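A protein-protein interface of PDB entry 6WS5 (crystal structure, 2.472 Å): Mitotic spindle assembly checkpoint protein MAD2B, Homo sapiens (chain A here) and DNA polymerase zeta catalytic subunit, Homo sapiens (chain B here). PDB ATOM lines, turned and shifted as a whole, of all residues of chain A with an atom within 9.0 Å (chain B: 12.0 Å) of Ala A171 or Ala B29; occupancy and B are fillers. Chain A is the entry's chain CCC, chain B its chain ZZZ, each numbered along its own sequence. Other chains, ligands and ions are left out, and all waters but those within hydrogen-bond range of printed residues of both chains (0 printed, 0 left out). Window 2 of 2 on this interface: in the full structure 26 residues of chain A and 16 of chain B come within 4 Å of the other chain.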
ATOM      1  N   ASP A  95      -0.568  12.096   8.471  1.00  0.00           N
ATOM      2  CA  ASP A  95      -1.752  11.265   8.896  1.00  0.00           C
ATOM      3  C   ASP A  95      -2.822  12.130   9.598  1.00  0.00           C
ATOM      4  O   ASP A  95      -3.914  11.631   9.924  1.00  0.00           O
ATOM      5  CB  ASP A  95      -1.324  10.143   9.861  1.00  0.00           C
ATOM      6  CG  ASP A  95      -0.828   8.833   9.236  1.00  0.00           C
ATOM      7  OD1 ASP A  95      -1.123   8.619   8.020  1.00  0.00           O
ATOM      8  OD2 ASP A  95      -0.190   8.002   9.972  1.00  0.00           O
ATOM      9  N   VAL A 166      -6.598  15.577  18.251  1.00  0.00           N
ATOM     10  CA  VAL A 166      -5.983  15.293  16.931  1.00  0.00           C
ATOM     11  C   VAL A 166      -7.015  14.567  16.083  1.00  0.00           C
ATOM     12  O   VAL A 166      -7.475  13.489  16.493  1.00  0.00           O
ATOM     13  CB  VAL A 166      -4.695  14.494  17.124  1.00  0.00           C
ATOM     14  CG1 VAL A 166      -4.206  13.870  15.840  1.00  0.00           C
ATOM     15  CG2 VAL A 166      -3.643  15.425  17.722  1.00  0.00           C
ATOM     16  N   HIS A 167      -7.476  15.217  15.008  1.00  0.00           N
ATOM     17  CA  HIS A 167      -8.252  14.572  13.913  1.00  0.00           C
ATOM     18  C   HIS A 167      -7.228  13.920  12.959  1.00  0.00           C
ATOM     19  O   HIS A 167      -6.368  14.654  12.467  1.00  0.00           O
ATOM     20  CB  HIS A 167      -9.140  15.615  13.243  1.00  0.00           C
ATOM     21  CG  HIS A 167     -10.285  16.060  14.081  1.00  0.00           C
ATOM     22  ND1 HIS A 167     -10.100  16.712  15.297  1.00  0.00           N
ATOM     23  CD2 HIS A 167     -11.603  15.876  13.965  1.00  0.00           C
ATOM     24  CE1 HIS A 167     -11.281  16.930  15.855  1.00  0.00           C
ATOM     25  NE2 HIS A 167     -12.210  16.450  15.079  1.00  0.00           N
ATOM     26  N   THR A 168      -7.237  12.599  12.803  1.00  0.00           N
ATOM     27  CA  THR A 168      -6.486  11.870  11.721  1.00  0.00           C
ATOM     28  C   THR A 168      -7.367  11.774  10.458  1.00  0.00           C
ATOM     29  O   THR A 168      -8.611  11.740  10.617  1.00  0.00           O
ATOM     30  CB  THR A 168      -6.121  10.425  12.121  1.00  0.00           C
ATOM     31  OG1 THR A 168      -7.309   9.762  12.680  1.00  0.00           O
ATOM     32  CG2 THR A 168      -4.923  10.398  13.045  1.00  0.00           C
ATOM     33  N   ARG A 169      -6.719  11.606   9.316  1.00  0.00           N
ATOM     34  CA  ARG A 169      -7.307  11.528   7.940  1.00  0.00           C
ATOM     35  C   ARG A 169      -8.293  10.359   7.842  1.00  0.00           C
ATOM     36  O   ARG A 169      -9.468  10.608   7.488  1.00  0.00           O
ATOM     37  CB  ARG A 169      -6.194  11.415   6.893  1.00  0.00           C
ATOM     38  CG  ARG A 169      -5.098  12.463   7.075  1.00  0.00           C
ATOM     39  CD  ARG A 169      -4.238  12.664   5.853  1.00  0.00           C
ATOM     40  NE  ARG A 169      -3.670  13.991   5.742  1.00  0.00           N
ATOM     41  CZ  ARG A 169      -4.376  15.092   5.510  1.00  0.00           C
ATOM     42  NH1 ARG A 169      -5.708  15.056   5.373  1.00  0.00           N
ATOM     43  NH2 ARG A 169      -3.723  16.237   5.448  1.00  0.00           N
ATOM     44  N   GLU A 170      -7.855   9.135   8.169  1.00  0.00           N
ATOM     45  CA  GLU A 170      -8.779   7.977   8.376  1.00  0.00           C
ATOM     46  C   GLU A 170      -8.419   7.286   9.708  1.00  0.00           C
ATOM     47  O   GLU A 170      -7.265   7.401  10.197  1.00  0.00           O
ATOM     48  CB  GLU A 170      -8.764   7.040   7.147  1.00  0.00           C
ATOM     49  CG  GLU A 170      -7.519   6.168   6.988  1.00  0.00           C
ATOM     50  CD  GLU A 170      -6.370   6.700   6.154  1.00  0.00           C
ATOM     51  OE1 GLU A 170      -5.442   5.882   5.846  1.00  0.00           O
ATOM     52  OE2 GLU A 170      -6.386   7.918   5.815  1.00  0.00           O
ATOM     53  N   ALA A 171      -9.385   6.621  10.315  1.00  0.00           N
ATOM     54  CA  ALA A 171      -9.230   5.738  11.478  1.00  0.00           C
ATOM     55  C   ALA A 171      -8.307   4.540  11.145  1.00  0.00           C
ATOM     56  O   ALA A 171      -8.519   3.850  10.223  1.00  0.00           O
ATOM     57  CB  ALA A 171     -10.614   5.297  11.934  1.00  0.00           C
ATOM     58  N   ALA A 172      -7.273   4.338  11.939  1.00  0.00           N
ATOM     59  CA  ALA A 172      -6.196   3.391  11.684  1.00  0.00           C
ATOM     60  C   ALA A 172      -5.481   3.095  13.004  1.00  0.00           C
ATOM     61  O   ALA A 172      -5.069   4.048  13.698  1.00  0.00           O
ATOM     62  CB  ALA A 172      -5.258   3.953  10.659  1.00  0.00           C
ATOM     63  N   THR A 173      -5.371   1.814  13.341  1.00  0.00           N
ATOM     64  CA  THR A 173      -4.549   1.338  14.463  1.00  0.00           C
ATOM     65  C   THR A 173      -3.128   1.884  14.351  1.00  0.00           C
ATOM     66  O   THR A 173      -2.556   2.205  15.439  1.00  0.00           O
ATOM     67  CB  THR A 173      -4.632  -0.185  14.558  1.00  0.00           C
ATOM     68  OG1 THR A 173      -4.065  -0.683  13.372  1.00  0.00           O
ATOM     69  CG2 THR A 173      -6.061  -0.680  14.681  1.00  0.00           C
ATOM     70  N   ARG A 174      -2.550   2.000  13.150  1.00  0.00           N
ATOM     71  CA  ARG A 174      -1.127   2.456  13.031  1.00  0.00           C
ATOM     72  C   ARG A 174      -1.007   3.821  13.734  1.00  0.00           C
ATOM     73  O   ARG A 174      -0.032   4.010  14.469  1.00  0.00           O
ATOM     74  CB  ARG A 174      -0.571   2.437  11.610  1.00  0.00           C
ATOM     75  CG  ARG A 174      -1.234   3.421  10.673  1.00  0.00           C
ATOM     76  CD  ARG A 174      -0.711   3.458   9.248  1.00  0.00           C
ATOM     77  NE  ARG A 174      -1.377   4.539   8.523  1.00  0.00           N
ATOM     78  CZ  ARG A 174      -2.558   4.428   7.891  1.00  0.00           C
ATOM     79  NH1 ARG A 174      -3.179   3.260   7.856  1.00  0.00           N
ATOM     80  NH2 ARG A 174      -3.108   5.481   7.282  1.00  0.00           N
ATOM     81  N   ASN A 175      -2.031   4.680  13.651  1.00  0.00           N
ATOM     82  CA  ASN A 175      -2.102   5.983  14.375  1.00  0.00           C
ATOM     83  C   ASN A 175      -1.949   5.801  15.888  1.00  0.00           C
ATOM     84  O   ASN A 175      -1.011   6.413  16.493  1.00  0.00           O
ATOM     85  CB  ASN A 175      -3.363   6.789  13.977  1.00  0.00           C
ATOM     86  CG  ASN A 175      -3.332   7.171  12.507  1.00  0.00           C
ATOM     87  OD1 ASN A 175      -2.206   7.409  11.990  1.00  0.00           O
ATOM     88  ND2 ASN A 175      -4.526   7.221  11.881  1.00  0.00           N
ATOM     89  N   MET A 176      -2.771   4.944  16.503  1.00  0.00           N
ATOM     90  CA  MET A 176      -2.740   4.731  17.978  1.00  0.00           C
ATOM     91  C   MET A 176      -1.467   4.051  18.381  1.00  0.00           C
ATOM     92  O   MET A 176      -1.029   4.334  19.502  1.00  0.00           O
ATOM     93  CB  MET A 176      -3.944   3.936  18.476  1.00  0.00           C
ATOM     94  CG  MET A 176      -5.121   4.857  18.698  1.00  0.00           C
ATOM     95  SD  MET A 176      -6.489   4.166  19.544  1.00  0.00           S
ATOM     96  CE  MET A 176      -5.716   3.383  20.945  1.00  0.00           C
ATOM     97  N   ILE A 188      -6.287   8.322  24.179  1.00  0.00           N
ATOM     98  CA  ILE A 188      -7.595   7.595  24.015  1.00  0.00           C
ATOM     99  C   ILE A 188      -8.371   8.255  22.856  1.00  0.00           C
ATOM    100  O   ILE A 188      -7.990   9.367  22.364  1.00  0.00           O
ATOM    101  CB  ILE A 188      -8.418   7.576  25.301  1.00  0.00           C
ATOM    102  CG1 ILE A 188      -8.874   8.995  25.740  1.00  0.00           C
ATOM    103  CG2 ILE A 188      -7.699   6.797  26.408  1.00  0.00           C
ATOM    104  CD1 ILE A 188      -9.655   9.052  26.999  1.00  0.00           C
ATOM    105  N   LEU A 189      -9.384   7.545  22.408  1.00  0.00           N
ATOM    106  CA  LEU A 189     -10.379   8.008  21.425  1.00  0.00           C
ATOM    107  C   LEU A 189     -11.337   8.940  22.179  1.00  0.00           C
ATOM    108  O   LEU A 189     -11.830   8.582  23.282  1.00  0.00           O
ATOM    109  CB  LEU A 189     -11.059   6.777  20.812  1.00  0.00           C
ATOM    110  CG  LEU A 189     -10.109   6.026  19.873  1.00  0.00           C
ATOM    111  CD1 LEU A 189     -10.475   4.588  19.694  1.00  0.00           C
ATOM    112  CD2 LEU A 189     -10.034   6.675  18.520  1.00  0.00           C
ATOM    113  N   ALA A 190     -11.552  10.126  21.645  1.00  0.00           N
ATOM    114  CA  ALA A 190     -12.198  11.219  22.399  1.00  0.00           C
ATOM    115  C   ALA A 190     -13.652  10.802  22.493  1.00  0.00           C
ATOM    116  O   ALA A 190     -14.049  10.026  21.620  1.00  0.00           O
ATOM    117  CB  ALA A 190     -11.990  12.544  21.696  1.00  0.00           C
ATOM    118  N   GLU A 192     -17.837  11.954  22.473  1.00  0.00           N
ATOM    119  CA  GLU A 192     -18.685  13.021  21.872  1.00  0.00           C
ATOM    120  C   GLU A 192     -18.792  14.182  22.869  1.00  0.00           C
ATOM    121  O   GLU A 192     -18.843  15.312  22.425  1.00  0.00           O
ATOM    122  CB  GLU A 192     -20.060  12.460  21.469  1.00  0.00           C
ATOM    123  CG  GLU A 192     -20.968  13.439  20.737  1.00  0.00           C
ATOM    124  CD  GLU A 192     -20.619  13.700  19.274  1.00  0.00           C
ATOM    125  OE1 GLU A 192     -19.839  12.914  18.720  1.00  0.00           O
ATOM    126  OE2 GLU A 192     -21.120  14.682  18.685  1.00  0.00           O
ATOM    127  N   ARG B  27     -19.465   6.542  16.289  1.00  0.00           N
ATOM    128  CA  ARG B  27     -18.760   6.063  15.075  1.00  0.00           C
ATOM    129  C   ARG B  27     -17.563   6.967  14.695  1.00  0.00           C
ATOM    130  O   ARG B  27     -17.172   6.972  13.499  1.00  0.00           O
ATOM    131  CB  ARG B  27     -19.816   6.003  13.966  1.00  0.00           C
ATOM    132  CG  ARG B  27     -20.571   7.313  13.807  1.00  0.00           C
ATOM    133  CD  ARG B  27     -21.450   7.396  12.577  1.00  0.00           C
ATOM    134  NE  ARG B  27     -21.847   8.791  12.446  1.00  0.00           N
ATOM    135  CZ  ARG B  27     -22.760   9.404  13.200  1.00  0.00           C
ATOM    136  NH1 ARG B  27     -23.433   8.752  14.133  1.00  0.00           N
ATOM    137  NH2 ARG B  27     -23.024  10.680  12.993  1.00  0.00           N
ATOM    138  N   THR B  28     -16.982   7.712  15.646  1.00  0.00           N
ATOM    139  CA  THR B  28     -15.934   8.749  15.389  1.00  0.00           C
ATOM    140  C   THR B  28     -14.578   8.281  15.929  1.00  0.00           C
ATOM    141  O   THR B  28     -14.148   8.834  16.993  1.00  0.00           O
ATOM    142  CB  THR B  28     -16.228  10.096  16.063  1.00  0.00           C
ATOM    143  OG1 THR B  28     -17.584  10.476  15.830  1.00  0.00           O
ATOM    144  CG2 THR B  28     -15.323  11.170  15.526  1.00  0.00           C
ATOM    145  N   ALA B  29     -13.895   7.374  15.190  1.00  0.00           N
ATOM    146  CA  ALA B  29     -12.689   6.690  15.680  1.00  0.00           C
ATOM    147  C   ALA B  29     -11.417   7.298  15.092  1.00  0.00           C
ATOM    148  O   ALA B  29     -10.314   6.688  15.304  1.00  0.00           O
ATOM    149  CB  ALA B  29     -12.837   5.203  15.446  1.00  0.00           C
ATOM    150  N   ASN B  30     -11.531   8.466  14.455  1.00  0.00           N
ATOM    151  CA  ASN B  30     -10.364   9.234  13.911  1.00  0.00           C
ATOM    152  C   ASN B  30      -9.958  10.420  14.800  1.00  0.00           C
ATOM    153  O   ASN B  30      -9.110  11.196  14.355  1.00  0.00           O
ATOM    154  CB  ASN B  30     -10.680   9.811  12.537  1.00  0.00           C
ATOM    155  CG  ASN B  30     -11.655  10.964  12.628  1.00  0.00           C
ATOM    156  OD1 ASN B  30     -12.775  10.814  13.125  1.00  0.00           O
ATOM    157  ND2 ASN B  30     -11.236  12.126  12.152  1.00  0.00           N
ATOM    158  N   ILE B  31     -10.563  10.580  15.988  1.00  0.00           N
ATOM    159  CA  ILE B  31     -10.258  11.661  16.980  1.00  0.00           C
ATOM    160  C   ILE B  31      -9.555  11.098  18.235  1.00  0.00           C
ATOM    161  O   ILE B  31     -10.197  10.250  19.032  1.00  0.00           O
ATOM    162  CB  ILE B  31     -11.528  12.453  17.270  1.00  0.00           C
ATOM    163  CG1 ILE B  31     -11.919  13.273  16.041  1.00  0.00           C
ATOM    164  CG2 ILE B  31     -11.343  13.342  18.492  1.00  0.00           C
ATOM    165  CD1 ILE B  31     -13.298  13.809  16.035  1.00  0.00           C
ATOM    166  N   LEU B  32      -8.287  11.537  18.422  1.00  0.00           N
ATOM    167  CA  LEU B  32      -7.422  11.126  19.552  1.00  0.00           C
ATOM    168  C   LEU B  32      -7.212  12.297  20.522  1.00  0.00           C
ATOM    169  O   LEU B  32      -7.274  13.486  20.133  1.00  0.00           O
ATOM    170  CB  LEU B  32      -6.085  10.615  19.001  1.00  0.00           C
ATOM    171  CG  LEU B  32      -6.146   9.305  18.228  1.00  0.00           C
ATOM    172  CD1 LEU B  32      -4.781   8.957  17.672  1.00  0.00           C
ATOM    173  CD2 LEU B  32      -6.673   8.203  19.116  1.00  0.00           C
ATOM    174  N   LYS B  33      -6.855  11.969  21.748  1.00  0.00           N
ATOM    175  CA  LYS B  33      -6.945  12.878  22.923  1.00  0.00           C
ATOM    176  C   LYS B  33      -6.034  12.306  23.990  1.00  0.00           C
ATOM    177  O   LYS B  33      -6.029  11.111  24.205  1.00  0.00           O
ATOM    178  CB  LYS B  33      -8.413  12.904  23.405  1.00  0.00           C
ATOM    179  CG  LYS B  33      -8.739  13.870  24.526  1.00  0.00           C
ATOM    180  CD  LYS B  33      -9.684  13.317  25.538  1.00  0.00           C
ATOM    181  CE  LYS B  33     -10.078  14.299  26.629  1.00  0.00           C
ATOM    182  NZ  LYS B  33      -8.934  14.792  27.464  1.00  0.00           N
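O of Val A166 sits at hydrogen-bond distance from N of Leu B32 (2.9 Å). The backbone NH of Ala A190 sits at hydrogen-bond distance from the backbone carbonyl oxygen of Ile B31, at 2.9 Å. N of Ile A188 is in hydrogen-bond range of O of Lys B33. O of Asn B30 sits at hydrogen-bond distance from N of Thr A168, 2.8 Å away.
The backbone carbonyl oxygen of Glu A170 sits at hydrogen-bond distance from the side-chain hydroxyl of Thr A168, at 3.4 Å.
Val A166 touches Asn B30 (O to O, 3.5 Å). Val A166 touches Ile B31. CA of His A167 touches O of Asn B30, at 3.5 Å. CD1 of Ile B31 touches NE2 of His A167 (3.0 Å). O of Ala B29 touches CB of Ala A171, 3.7 Å away. Met A176 touches Leu B32. O of Ile A188 touches CA of Leu B32, 3.4 Å away. Ile B31 touches Leu A189 (O to CA, 3.3 Å). Leu A189 touches Leu B32 (CD2 to CD2, 3.7 Å). Lys B33 touches Ala A190 (CB to CB, 3.98 Å).
Of the printed residues of chain B, Val A166 touches Asn B30, Ile B31 and Leu B32. Printed residues of chain B within 4 Å of His A167: Asn B30 (3.5 Å) and Ile B31 (3.0 Å). Of chain B, only Asn B30 (2.8 Å) comes within 4 Å of Thr A168. Arg A169 touches none of the printed residues of chain B. Glu A170 touches none of the printed residues of chain B. Of chain B, only Ala B29 (3.7 Å) comes within 4 Å of Ala A171. No residue of chain B comes within 4 Å of Ala A172. Asn A175 touches none of the printed residues of chain B. Of chain A, only Ala A171 (3.7 Å) and Leu A189 (3.2 Å) come within 4 Å of Ala B29. The nearest printed residue of chain A that does not touch Ile B31 is Ile A188 (4.1 Å).
Of the 16 printed residues of chain A, 8 touch a printed residue of chain B. Printed residues of chain A that touch a printed residue of chain B: Val A166, His A167, Thr A168, Ala A171, Met A176, Ile A188, Leu A189 and Ala A190. Hydrophobic or aromatic side chains of chain A that line the printed part of chain B: His A167, Ala A171, Met A176, Ile A188, Leu A189 and Ala A190. Of the 7 printed residues of chain B, 5 touch a printed residue of chain A. Hydrophobic or aromatic side chains of chain B that line the printed part of chain A: Ile B31 and Leu B32. Among the printed residues, 15 pairs touch across the chains.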
